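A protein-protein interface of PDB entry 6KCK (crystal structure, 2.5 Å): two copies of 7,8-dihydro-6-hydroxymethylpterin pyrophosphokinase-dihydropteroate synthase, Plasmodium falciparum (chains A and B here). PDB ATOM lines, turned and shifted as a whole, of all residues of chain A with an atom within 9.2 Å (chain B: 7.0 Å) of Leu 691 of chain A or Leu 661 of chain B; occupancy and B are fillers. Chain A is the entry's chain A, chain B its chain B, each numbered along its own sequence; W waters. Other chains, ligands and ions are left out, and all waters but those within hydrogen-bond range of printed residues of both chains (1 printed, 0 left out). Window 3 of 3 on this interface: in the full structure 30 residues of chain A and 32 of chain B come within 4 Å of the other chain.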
ATOM      1  N   ILE A 391       4.452 -12.920 -23.182  1.00  0.00           N
ATOM      2  CA  ILE A 391       3.992 -11.625 -23.636  1.00  0.00           C
ATOM      3  C   ILE A 391       4.603 -11.295 -24.993  1.00  0.00           C
ATOM      4  O   ILE A 391       5.814 -11.418 -25.187  1.00  0.00           O
ATOM      5  CB  ILE A 391       4.383 -10.523 -22.650  1.00  0.00           C
ATOM      6  CG1 ILE A 391       3.691 -10.781 -21.313  1.00  0.00           C
ATOM      7  CG2 ILE A 391       4.073  -9.119 -23.225  1.00  0.00           C
ATOM      8  CD1 ILE A 391       4.055  -9.795 -20.242  1.00  0.00           C
ATOM      9  N   GLY A 393       4.984  -8.133 -27.355  1.00  0.00           N
ATOM     10  CA  GLY A 393       4.821  -6.668 -27.385  1.00  0.00           C
ATOM     11  C   GLY A 393       4.533  -6.140 -28.779  1.00  0.00           C
ATOM     12  O   GLY A 393       5.177  -6.536 -29.769  1.00  0.00           O
ATOM     13  N   ARG A 417      11.614   2.066 -28.606  1.00  0.00           N
ATOM     14  CA  ARG A 417      10.440   1.388 -28.087  1.00  0.00           C
ATOM     15  C   ARG A 417      10.654  -0.144 -28.008  1.00  0.00           C
ATOM     16  O   ARG A 417      10.349  -0.771 -26.981  1.00  0.00           O
ATOM     17  CB  ARG A 417       9.201   1.795 -28.884  1.00  0.00           C
ATOM     18  CG  ARG A 417       7.922   1.136 -28.438  1.00  0.00           C
ATOM     19  CD  ARG A 417       7.611   1.321 -26.962  1.00  0.00           C
ATOM     20  NE  ARG A 417       6.410   0.567 -26.567  1.00  0.00           N
ATOM     21  CZ  ARG A 417       6.097   0.250 -25.309  1.00  0.00           C
ATOM     22  NH1 ARG A 417       6.880   0.637 -24.298  1.00  0.00           N
ATOM     23  NH2 ARG A 417       4.993  -0.436 -25.047  1.00  0.00           N
ATOM     24  N   GLU A 420      12.661  -0.661 -24.937  1.00  0.00           N
ATOM     25  CA  GLU A 420      11.809  -0.470 -23.785  1.00  0.00           C
ATOM     26  C   GLU A 420      10.957  -1.728 -23.493  1.00  0.00           C
ATOM     27  O   GLU A 420      10.738  -2.067 -22.331  1.00  0.00           O
ATOM     28  CB  GLU A 420      10.931   0.742 -23.987  1.00  0.00           C
ATOM     29  CG  GLU A 420      10.467   1.396 -22.701  1.00  0.00           C
ATOM     30  CD  GLU A 420       9.525   2.548 -22.965  1.00  0.00           C
ATOM     31  OE1 GLU A 420       9.301   2.884 -24.147  1.00  0.00           O
ATOM     32  OE2 GLU A 420       9.013   3.133 -21.991  1.00  0.00           O
ATOM     33  N   MET A 421      10.521  -2.433 -24.543  1.00  0.00           N
ATOM     34  CA  MET A 421       9.646  -3.601 -24.407  1.00  0.00           C
ATOM     35  C   MET A 421      10.403  -4.842 -23.967  1.00  0.00           C
ATOM     36  O   MET A 421       9.894  -5.612 -23.135  1.00  0.00           O
ATOM     37  CB  MET A 421       8.880  -3.871 -25.698  1.00  0.00           C
ATOM     38  CG  MET A 421       7.715  -2.927 -25.921  1.00  0.00           C
ATOM     39  SD  MET A 421       6.738  -3.367 -27.381  1.00  0.00           S
ATOM     40  CE  MET A 421       7.834  -3.021 -28.733  1.00  0.00           C
ATOM     41  N   ILE A 422      11.610  -5.041 -24.500  1.00  0.00           N
ATOM     42  CA  ILE A 422      12.479  -6.107 -23.982  1.00  0.00           C
ATOM     43  C   ILE A 422      12.669  -5.951 -22.464  1.00  0.00           C
ATOM     44  O   ILE A 422      12.494  -6.905 -21.704  1.00  0.00           O
ATOM     45  CB  ILE A 422      13.865  -6.177 -24.675  1.00  0.00           C
ATOM     46  CG1 ILE A 422      13.718  -6.364 -26.187  1.00  0.00           C
ATOM     47  CG2 ILE A 422      14.665  -7.375 -24.158  1.00  0.00           C
ATOM     48  CD1 ILE A 422      15.020  -6.188 -26.934  1.00  0.00           C
ATOM     49  N   ASN A 423      12.992  -4.743 -22.022  1.00  0.00           N
ATOM     50  CA  ASN A 423      13.271  -4.530 -20.610  1.00  0.00           C
ATOM     51  C   ASN A 423      12.005  -4.494 -19.756  1.00  0.00           C
ATOM     52  O   ASN A 423      12.084  -4.682 -18.547  1.00  0.00           O
ATOM     53  CB  ASN A 423      14.154  -3.285 -20.397  1.00  0.00           C
ATOM     54  CG  ASN A 423      15.567  -3.483 -20.948  1.00  0.00           C
ATOM     55  OD1 ASN A 423      16.271  -4.451 -20.575  1.00  0.00           O
ATOM     56  ND2 ASN A 423      15.987  -2.587 -21.866  1.00  0.00           N
ATOM     57  N   GLU A 424      10.850  -4.251 -20.381  1.00  0.00           N
ATOM     58  CA  GLU A 424       9.602  -4.320 -19.652  1.00  0.00           C
ATOM     59  C   GLU A 424       9.099  -5.769 -19.561  1.00  0.00           C
ATOM     60  O   GLU A 424       8.166  -6.043 -18.827  1.00  0.00           O
ATOM     61  CB  GLU A 424       8.546  -3.412 -20.247  1.00  0.00           C
ATOM     62  CG  GLU A 424       8.907  -1.944 -20.251  1.00  0.00           C
ATOM     63  CD  GLU A 424       7.790  -1.052 -20.794  1.00  0.00           C
ATOM     64  OE1 GLU A 424       6.779  -1.577 -21.309  1.00  0.00           O
ATOM     65  OE2 GLU A 424       7.910   0.196 -20.696  1.00  0.00           O
ATOM     66  N   GLY A 425       9.718  -6.698 -20.291  1.00  0.00           N
ATOM     67  CA  GLY A 425       9.370  -8.126 -20.157  1.00  0.00           C
ATOM     68  C   GLY A 425       8.846  -8.934 -21.350  1.00  0.00           C
ATOM     69  O   GLY A 425       8.583 -10.137 -21.196  1.00  0.00           O
ATOM     70  N   ALA A 426       8.698  -8.296 -22.525  1.00  0.00           N
ATOM     71  CA  ALA A 426       8.246  -8.963 -23.761  1.00  0.00           C
ATOM     72  C   ALA A 426       9.222 -10.056 -24.222  1.00  0.00           C
ATOM     73  O   ALA A 426      10.408  -9.806 -24.324  1.00  0.00           O
ATOM     74  CB  ALA A 426       8.022  -7.938 -24.867  1.00  0.00           C
ATOM     75  N   ILE A 667      -6.958  -0.412 -21.143  1.00  0.00           N
ATOM     76  CA  ILE A 667      -5.765  -1.061 -20.667  1.00  0.00           C
ATOM     77  C   ILE A 667      -6.148  -2.020 -19.527  1.00  0.00           C
ATOM     78  O   ILE A 667      -5.764  -3.196 -19.570  1.00  0.00           O
ATOM     79  CB  ILE A 667      -4.668  -0.052 -20.279  1.00  0.00           C
ATOM     80  CG1 ILE A 667      -4.238   0.706 -21.539  1.00  0.00           C
ATOM     81  CG2 ILE A 667      -3.475  -0.761 -19.643  1.00  0.00           C
ATOM     82  CD1 ILE A 667      -3.216   1.794 -21.295  1.00  0.00           C
ATOM     83  N   LEU A 671      -5.999  -6.223 -18.756  1.00  0.00           N
ATOM     84  CA  LEU A 671      -5.320  -6.924 -17.664  1.00  0.00           C
ATOM     85  C   LEU A 671      -6.202  -8.037 -17.111  1.00  0.00           C
ATOM     86  O   LEU A 671      -5.681  -9.099 -16.792  1.00  0.00           O
ATOM     87  CB  LEU A 671      -4.832  -5.967 -16.587  1.00  0.00           C
ATOM     88  CG  LEU A 671      -3.886  -4.930 -17.237  1.00  0.00           C
ATOM     89  CD1 LEU A 671      -3.625  -3.803 -16.242  1.00  0.00           C
ATOM     90  CD2 LEU A 671      -2.596  -5.568 -17.750  1.00  0.00           C
ATOM     91  N   VAL A 687       0.089  -7.772 -26.853  1.00  0.00           N
ATOM     92  CA  VAL A 687      -0.368  -6.645 -26.033  1.00  0.00           C
ATOM     93  C   VAL A 687       0.451  -5.361 -26.348  1.00  0.00           C
ATOM     94  O   VAL A 687       1.633  -5.447 -26.713  1.00  0.00           O
ATOM     95  CB  VAL A 687      -0.290  -6.977 -24.480  1.00  0.00           C
ATOM     96  CG1 VAL A 687      -1.137  -8.176 -24.083  1.00  0.00           C
ATOM     97  CG2 VAL A 687       1.119  -7.231 -24.011  1.00  0.00           C
ATOM     98  N   HIS A 688      -0.182  -4.190 -26.209  1.00  0.00           N
ATOM     99  CA  HIS A 688       0.538  -2.892 -26.196  1.00  0.00           C
ATOM    100  C   HIS A 688       1.205  -2.599 -24.910  1.00  0.00           C
ATOM    101  O   HIS A 688       2.278  -2.030 -24.897  1.00  0.00           O
ATOM    102  CB  HIS A 688      -0.406  -1.757 -26.436  1.00  0.00           C
ATOM    103  CG  HIS A 688      -1.128  -1.865 -27.717  1.00  0.00           C
ATOM    104  ND1 HIS A 688      -2.289  -2.561 -27.834  1.00  0.00           N
ATOM    105  CD2 HIS A 688      -0.800  -1.402 -28.994  1.00  0.00           C
ATOM    106  CE1 HIS A 688      -2.701  -2.513 -29.118  1.00  0.00           C
ATOM    107  NE2 HIS A 688      -1.782  -1.800 -29.827  1.00  0.00           N
ATOM    108  N   ASP A 689       0.557  -2.951 -23.801  1.00  0.00           N
ATOM    109  CA  ASP A 689       1.019  -2.520 -22.478  1.00  0.00           C
ATOM    110  C   ASP A 689       1.828  -3.625 -21.819  1.00  0.00           C
ATOM    111  O   ASP A 689       1.302  -4.451 -21.048  1.00  0.00           O
ATOM    112  CB  ASP A 689      -0.198  -2.073 -21.659  1.00  0.00           C
ATOM    113  CG  ASP A 689      -1.025  -0.992 -22.392  1.00  0.00           C
ATOM    114  OD1 ASP A 689      -0.513   0.139 -22.574  1.00  0.00           O
ATOM    115  OD2 ASP A 689      -2.175  -1.251 -22.795  1.00  0.00           O
ATOM    116  N   VAL A 690       3.113  -3.648 -22.142  1.00  0.00           N
ATOM    117  CA  VAL A 690       4.007  -4.718 -21.701  1.00  0.00           C
ATOM    118  C   VAL A 690       4.249  -4.687 -20.208  1.00  0.00           C
ATOM    119  O   VAL A 690       4.087  -5.723 -19.539  1.00  0.00           O
ATOM    120  CB  VAL A 690       5.352  -4.764 -22.472  1.00  0.00           C
ATOM    121  CG1 VAL A 690       6.198  -5.963 -22.042  1.00  0.00           C
ATOM    122  CG2 VAL A 690       5.097  -4.839 -23.968  1.00  0.00           C
ATOM    123  N   LEU A 691       4.607  -3.516 -19.678  1.00  0.00           N
ATOM    124  CA  LEU A 691       4.940  -3.389 -18.253  1.00  0.00           C
ATOM    125  C   LEU A 691       3.773  -3.874 -17.406  1.00  0.00           C
ATOM    126  O   LEU A 691       3.943  -4.728 -16.512  1.00  0.00           O
ATOM    127  CB  LEU A 691       5.272  -1.944 -17.881  1.00  0.00           C
ATOM    128  CG  LEU A 691       5.720  -1.714 -16.428  1.00  0.00           C
ATOM    129  CD1 LEU A 691       6.740  -0.594 -16.368  1.00  0.00           C
ATOM    130  CD2 LEU A 691       4.539  -1.372 -15.521  1.00  0.00           C
ATOM    131  N   GLU A 692       2.595  -3.341 -17.712  1.00  0.00           N
ATOM    132  CA  GLU A 692       1.397  -3.649 -16.969  1.00  0.00           C
ATOM    133  C   GLU A 692       1.105  -5.153 -17.031  1.00  0.00           C
ATOM    134  O   GLU A 692       0.820  -5.767 -16.011  1.00  0.00           O
ATOM    135  CB  GLU A 692       0.225  -2.820 -17.481  1.00  0.00           C
ATOM    136  CG  GLU A 692       0.458  -1.307 -17.392  1.00  0.00           C
ATOM    137  CD  GLU A 692       1.392  -0.733 -18.478  1.00  0.00           C
ATOM    138  OE1 GLU A 692       2.026  -1.498 -19.253  1.00  0.00           O
ATOM    139  OE2 GLU A 692       1.513   0.510 -18.545  1.00  0.00           O
ATOM    140  N   THR A 693       1.243  -5.739 -18.217  1.00  0.00           N
ATOM    141  CA  THR A 693       0.922  -7.146 -18.406  1.00  0.00           C
ATOM    142  C   THR A 693       1.885  -8.012 -17.605  1.00  0.00           C
ATOM    143  O   THR A 693       1.453  -8.968 -16.965  1.00  0.00           O
ATOM    144  CB  THR A 693       0.833  -7.556 -19.926  1.00  0.00           C
ATOM    145  OG1 THR A 693      -0.178  -6.793 -20.579  1.00  0.00           O
ATOM    146  CG2 THR A 693       0.421  -8.978 -20.091  1.00  0.00           C
ATOM    147  N   LYS A 694       3.171  -7.667 -17.624  1.00  0.00           N
ATOM    148  CA  LYS A 694       4.220  -8.398 -16.873  1.00  0.00           C
ATOM    149  C   LYS A 694       3.973  -8.369 -15.369  1.00  0.00           C
ATOM    150  O   LYS A 694       4.093  -9.396 -14.701  1.00  0.00           O
ATOM    151  CB  LYS A 694       5.643  -7.897 -17.198  1.00  0.00           C
ATOM    152  CG  LYS A 694       6.768  -8.775 -16.657  1.00  0.00           C
ATOM    153  CD  LYS A 694       6.903 -10.058 -17.487  1.00  0.00           C
ATOM    154  CE  LYS A 694       7.911 -11.056 -16.904  1.00  0.00           C
ATOM    155  NZ  LYS A 694       8.885 -10.407 -15.967  1.00  0.00           N
ATOM    156  N   SER A 695       3.611  -7.201 -14.850  1.00  0.00           N
ATOM    157  CA  SER A 695       3.229  -7.066 -13.447  1.00  0.00           C
ATOM    158  C   SER A 695       2.123  -8.025 -13.053  1.00  0.00           C
ATOM    159  O   SER A 695       2.198  -8.687 -11.988  1.00  0.00           O
ATOM    160  CB  SER A 695       2.787  -5.660 -13.163  1.00  0.00           C
ATOM    161  OG  SER A 695       3.864  -4.778 -13.399  1.00  0.00           O
ATOM    162  N   VAL A 696       1.112  -8.140 -13.910  1.00  0.00           N
ATOM    163  CA  VAL A 696       0.000  -9.010 -13.607  1.00  0.00           C
ATOM    164  C   VAL A 696       0.500 -10.428 -13.607  1.00  0.00           C
ATOM    165  O   VAL A 696       0.269 -11.151 -12.654  1.00  0.00           O
ATOM    166  CB  VAL A 696      -1.211  -8.805 -14.551  1.00  0.00           C
ATOM    167  CG1 VAL A 696      -2.161  -9.988 -14.441  1.00  0.00           C
ATOM    168  CG2 VAL A 696      -1.947  -7.511 -14.201  1.00  0.00           C
ATOM    169  N   LEU A 697       1.229 -10.833 -14.631  1.00  0.00           N
ATOM    170  CA  LEU A 697       1.600 -12.263 -14.742  1.00  0.00           C
ATOM    171  C   LEU A 697       2.568 -12.665 -13.644  1.00  0.00           C
ATOM    172  O   LEU A 697       2.503 -13.793 -13.136  1.00  0.00           O
ATOM    173  CB  LEU A 697       2.150 -12.599 -16.139  1.00  0.00           C
ATOM    174  CG  LEU A 697       1.178 -12.424 -17.336  1.00  0.00           C
ATOM    175  CD1 LEU A 697       1.849 -12.852 -18.640  1.00  0.00           C
ATOM    176  CD2 LEU A 697      -0.107 -13.223 -17.148  1.00  0.00           C
ATOM    177  N   ASP A 698       3.455 -11.741 -13.257  1.00  0.00           N
ATOM    178  CA  ASP A 698       4.380 -11.973 -12.147  1.00  0.00           C
ATOM    179  C   ASP A 698       3.622 -12.193 -10.842  1.00  0.00           C
ATOM    180  O   ASP A 698       3.880 -13.159 -10.096  1.00  0.00           O
ATOM    181  CB  ASP A 698       5.358 -10.805 -11.999  1.00  0.00           C
ATOM    182  CG  ASP A 698       6.532 -10.886 -12.975  1.00  0.00           C
ATOM    183  OD1 ASP A 698       6.679 -11.865 -13.753  1.00  0.00           O
ATOM    184  OD2 ASP A 698       7.332  -9.937 -12.966  1.00  0.00           O
ATOM    185  N   VAL A 699       2.652 -11.330 -10.565  1.00  0.00           N
ATOM    186  CA  VAL A 699       1.909 -11.534  -9.337  1.00  0.00           C
ATOM    187  C   VAL A 699       1.217 -12.889  -9.328  1.00  0.00           C
ATOM    188  O   VAL A 699       1.312 -13.604  -8.340  1.00  0.00           O
ATOM    189  CB  VAL A 699       0.919 -10.426  -9.020  1.00  0.00           C
ATOM    190  CG1 VAL A 699       0.082 -10.834  -7.824  1.00  0.00           C
ATOM    191  CG2 VAL A 699       1.654  -9.132  -8.735  1.00  0.00           C
ATOM    192  N   MET B 616       7.447  -8.892  -8.063  1.00  0.00           N
ATOM    193  CA  MET B 616       8.074  -8.490  -9.326  1.00  0.00           C
ATOM    194  C   MET B 616       9.552  -8.854  -9.447  1.00  0.00           C
ATOM    195  O   MET B 616      10.185  -9.320  -8.489  1.00  0.00           O
ATOM    196  CB  MET B 616       7.978  -6.976  -9.514  1.00  0.00           C
ATOM    197  CG  MET B 616       6.655  -6.330  -9.151  1.00  0.00           C
ATOM    198  SD  MET B 616       5.257  -6.800 -10.170  1.00  0.00           S
ATOM    199  CE  MET B 616       4.062  -5.643  -9.516  1.00  0.00           C
ATOM    200  N   ASP B 657      11.097   9.013 -12.773  1.00  0.00           N
ATOM    201  CA  ASP B 657      10.300   8.010 -13.477  1.00  0.00           C
ATOM    202  C   ASP B 657      10.857   6.594 -13.341  1.00  0.00           C
ATOM    203  O   ASP B 657      10.671   5.753 -14.223  1.00  0.00           O
ATOM    204  CB  ASP B 657      10.119   8.383 -14.955  1.00  0.00           C
ATOM    205  CG  ASP B 657       8.802   9.096 -15.222  1.00  0.00           C
ATOM    206  OD1 ASP B 657       8.050   9.366 -14.260  1.00  0.00           O
ATOM    207  OD2 ASP B 657       8.516   9.389 -16.403  1.00  0.00           O
ATOM    208  N   LYS B 658      11.545   6.347 -12.229  1.00  0.00           N
ATOM    209  CA  LYS B 658      11.924   4.994 -11.821  1.00  0.00           C
ATOM    210  C   LYS B 658      10.987   4.528 -10.703  1.00  0.00           C
ATOM    211  O   LYS B 658      10.716   3.333 -10.573  1.00  0.00           O
ATOM    212  CB  LYS B 658      13.388   4.938 -11.366  1.00  0.00           C
ATOM    213  CG  LYS B 658      14.396   5.199 -12.478  1.00  0.00           C
ATOM    214  CD  LYS B 658      15.805   5.384 -11.932  1.00  0.00           C
ATOM    215  CE  LYS B 658      16.773   5.767 -13.039  1.00  0.00           C
ATOM    216  NZ  LYS B 658      18.147   6.002 -12.517  1.00  0.00           N
ATOM    217  N   ASP B 659      10.495   5.488  -9.913  1.00  0.00           N
ATOM    218  CA  ASP B 659       9.495   5.244  -8.870  1.00  0.00           C
ATOM    219  C   ASP B 659       8.073   5.247  -9.437  1.00  0.00           C
ATOM    220  O   ASP B 659       7.141   4.741  -8.805  1.00  0.00           O
ATOM    221  CB  ASP B 659       9.612   6.287  -7.751  1.00  0.00           C
ATOM    222  CG  ASP B 659      10.852   6.093  -6.887  1.00  0.00           C
ATOM    223  OD1 ASP B 659      11.374   4.958  -6.800  1.00  0.00           O
ATOM    224  OD2 ASP B 659      11.304   7.089  -6.283  1.00  0.00           O
ATOM    225  N   GLN B 660       7.913   5.836 -10.619  1.00  0.00           N
ATOM    226  CA  GLN B 660       6.634   5.813 -11.320  1.00  0.00           C
ATOM    227  C   GLN B 660       6.374   4.455 -11.968  1.00  0.00           C
ATOM    228  O   GLN B 660       5.251   3.962 -11.937  1.00  0.00           O
ATOM    229  CB  GLN B 660       6.543   6.932 -12.362  1.00  0.00           C
ATOM    230  CG  GLN B 660       5.911   8.209 -11.835  1.00  0.00           C
ATOM    231  CD  GLN B 660       5.002   8.876 -12.853  1.00  0.00           C
ATOM    232  OE1 GLN B 660       5.124   8.647 -14.060  1.00  0.00           O
ATOM    233  NE2 GLN B 660       4.082   9.709 -12.368  1.00  0.00           N
ATOM    234  N   LEU B 661       7.415   3.866 -12.558  1.00  0.00           N
ATOM    235  CA  LEU B 661       7.352   2.495 -13.051  1.00  0.00           C
ATOM    236  C   LEU B 661       7.015   1.575 -11.893  1.00  0.00           C
ATOM    237  O   LEU B 661       6.252   0.629 -12.055  1.00  0.00           O
ATOM    238  CB  LEU B 661       8.679   2.055 -13.684  1.00  0.00           C
ATOM    239  CG  LEU B 661       9.217   2.824 -14.895  1.00  0.00           C
ATOM    240  CD1 LEU B 661      10.612   2.324 -15.235  1.00  0.00           C
ATOM    241  CD2 LEU B 661       8.292   2.743 -16.107  1.00  0.00           C
ATOM    242  N   LEU B 662       7.580   1.865 -10.723  1.00  0.00           N
ATOM    243  CA  LEU B 662       7.325   1.065  -9.526  1.00  0.00           C
ATOM    244  C   LEU B 662       5.896   1.252  -8.977  1.00  0.00           C
ATOM    245  O   LEU B 662       5.264   0.287  -8.544  1.00  0.00           O
ATOM    246  CB  LEU B 662       8.411   1.299  -8.462  1.00  0.00           C
ATOM    247  CG  LEU B 662       9.828   0.802  -8.831  1.00  0.00           C
ATOM    248  CD1 LEU B 662      10.896   1.479  -7.973  1.00  0.00           C
ATOM    249  CD2 LEU B 662       9.990  -0.724  -8.811  1.00  0.00           C
ATOM    250  N   TYR B 663       5.378   2.476  -9.026  1.00  0.00           N
ATOM    251  CA  TYR B 663       3.986   2.706  -8.667  1.00  0.00           C
ATOM    252  C   TYR B 663       2.975   2.237  -9.719  1.00  0.00           C
ATOM    253  O   TYR B 663       1.839   1.895  -9.390  1.00  0.00           O
ATOM    254  CB  TYR B 663       3.734   4.148  -8.217  1.00  0.00           C
ATOM    255  CG  TYR B 663       3.473   4.205  -6.720  1.00  0.00           C
ATOM    256  CD1 TYR B 663       2.362   3.539  -6.163  1.00  0.00           C
ATOM    257  CD2 TYR B 663       4.335   4.883  -5.852  1.00  0.00           C
ATOM    258  CE1 TYR B 663       2.110   3.560  -4.803  1.00  0.00           C
ATOM    259  CE2 TYR B 663       4.084   4.912  -4.481  1.00  0.00           C
ATOM    260  CZ  TYR B 663       2.968   4.251  -3.968  1.00  0.00           C
ATOM    261  OH  TYR B 663       2.699   4.265  -2.619  1.00  0.00           O
ATOM    262  N   GLN B 664       3.399   2.190 -10.975  1.00  0.00           N
ATOM    263  CA  GLN B 664       2.588   1.602 -12.027  1.00  0.00           C
ATOM    264  C   GLN B 664       2.510   0.091 -11.806  1.00  0.00           C
ATOM    265  O   GLN B 664       1.444  -0.512 -11.902  1.00  0.00           O
ATOM    266  CB  GLN B 664       3.190   1.932 -13.400  1.00  0.00           C
ATOM    267  CG  GLN B 664       2.476   1.334 -14.599  1.00  0.00           C
ATOM    268  CD  GLN B 664       1.198   2.064 -15.006  1.00  0.00           C
ATOM    269  OE1 GLN B 664       0.523   2.685 -14.184  1.00  0.00           O
ATOM    270  NE2 GLN B 664       0.853   1.973 -16.294  1.00  0.00           N
ATOM    271  N   LYS B 665       3.667  -0.497 -11.534  1.00  0.00           N
ATOM    272  CA  LYS B 665       3.810  -1.914 -11.341  1.00  0.00           C
ATOM    273  C   LYS B 665       2.937  -2.321 -10.167  1.00  0.00           C
ATOM    274  O   LYS B 665       2.267  -3.362 -10.178  1.00  0.00           O
ATOM    275  CB  LYS B 665       5.264  -2.254 -11.048  1.00  0.00           C
ATOM    276  CG  LYS B 665       6.178  -2.344 -12.265  1.00  0.00           C
ATOM    277  CD  LYS B 665       7.550  -2.863 -11.839  1.00  0.00           C
ATOM    278  CE  LYS B 665       8.551  -2.948 -12.979  1.00  0.00           C
ATOM    279  NZ  LYS B 665       9.299  -4.234 -12.852  1.00  0.00           N
ATOM    280  N   ASN B 666       2.896  -1.452  -9.179  1.00  0.00           N
ATOM    281  CA  ASN B 666       2.139  -1.734  -8.005  1.00  0.00           C
ATOM    282  C   ASN B 666       0.592  -1.684  -8.185  1.00  0.00           C
ATOM    283  O   ASN B 666      -0.089  -2.594  -7.714  1.00  0.00           O
ATOM    284  CB  ASN B 666       2.662  -0.891  -6.837  1.00  0.00           C
ATOM    285  CG  ASN B 666       2.411  -1.544  -5.506  1.00  0.00           C
ATOM    286  OD1 ASN B 666       1.368  -1.337  -4.911  1.00  0.00           O
ATOM    287  ND2 ASN B 666       3.353  -2.353  -5.040  1.00  0.00           N
ATOM    288  N   CYS B 668      -0.926  -2.216 -11.064  1.00  0.00           N
ATOM    289  CA  CYS B 668      -1.120  -3.379 -11.906  1.00  0.00           C
ATOM    290  C   CYS B 668      -1.022  -4.732 -11.153  1.00  0.00           C
ATOM    291  O   CYS B 668      -1.868  -5.633 -11.343  1.00  0.00           O
ATOM    292  CB  CYS B 668      -0.201  -3.297 -13.136  1.00  0.00           C
ATOM    293  SG  CYS B 668      -0.648  -1.878 -14.192  1.00  0.00           S
HETATM  294  O   HOH W   1       6.319  -5.634 -13.921  1.00  0.00           O
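Of the 12 printed residues of chain B, 5 touch a printed residue of chain A. Hydrophobic or aromatic side chains of chain A that line the printed part of chain B: Leu 691 and Val 696. Among the printed residues, 10 pairs touch across the chains. Among the printed residues, no Asp or Glu carboxylate lies within 4 Å of a Lys or Arg side-chain nitrogen of the other chain.
His 688 of chain A touches none of the printed residues of chain B. Leu 691 of chain A touches just these residues of chain B: Leu 661, Gln 664 and Lys 665. Of the printed residues of chain B, Ser 695 of chain A touches Met 616, Lys 665 and Cys 668. Of the printed residues of chain B, Asp 698 of chain A touches Met 616. Of the printed residues of chain A, Leu 661 of chain B touches Leu 691 (3.7 Å). Printed residues of chain A within 4 Å of Gln 664 of chain B: Leu 691 and Glu 692. Of the printed residues of chain A, Lys 665 of chain B touches Leu 691 (3.8 Å) and Ser 695 (3.5 Å). Printed residues of chain A within 4 Å of Cys 668 of chain B: Glu 692, Ser 695 and Val 696. The nearest printed residue of chain A that does not touch Met 616 of chain B is Val 699 of chain A (4.3 Å).
The side-chain carboxylate of Glu 424 of chain A lies within hydrogen-bond range of the backbone NH of Leu 691 of chain A, at 3.3 Å. The backbone carbonyl oxygen (O) of Leu 691 of chain A is in hydrogen-bond range of the side-chain hydroxyl (OG) of Ser 695 of chain A (3.1 Å). The side-chain amino group (NZ) of Lys 694 of chain A is in salt-bridge range of the side-chain carboxylate (OD2) of Asp 698 of chain A (3.4 Å). The backbone carbonyl oxygen of Gln 664 of chain B lies within hydrogen-bond range of the side-chain sulfur of Cys 668 of chain B (3.4 Å).
No position is printed for both chains. Of the 10 pairs that touch across the chains among the printed residues, none has its exchanged pair printed and touching as well.
Water W1 bridges OG of Ser 695 of chain A and NZ of Lys 665 of chain B.
OE2 of Glu 692 of chain A sits at hydrogen-bond distance from NE2 of Gln 664 of chain B, at 2.8 Å.
Among the printed residues, merely in contact across the chains: Leu 691 of chain A with Leu 661 of chain B, Leu 691 of chain A with Gln 664 of chain B, Leu 691 of chain A with Lys 665 of chain B, Glu 692 of chain A with Cys 668 of chain B, Ser 695 of chain A with Met 616 of chain B, Ser 695 of chain A with Lys 665 of chain B, Ser 695 of chain A with Cys 668 of chain B, Val 696 of chain A with Cys 668 of chain B and Asp 698 of chain A with Met 616 of chain B.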
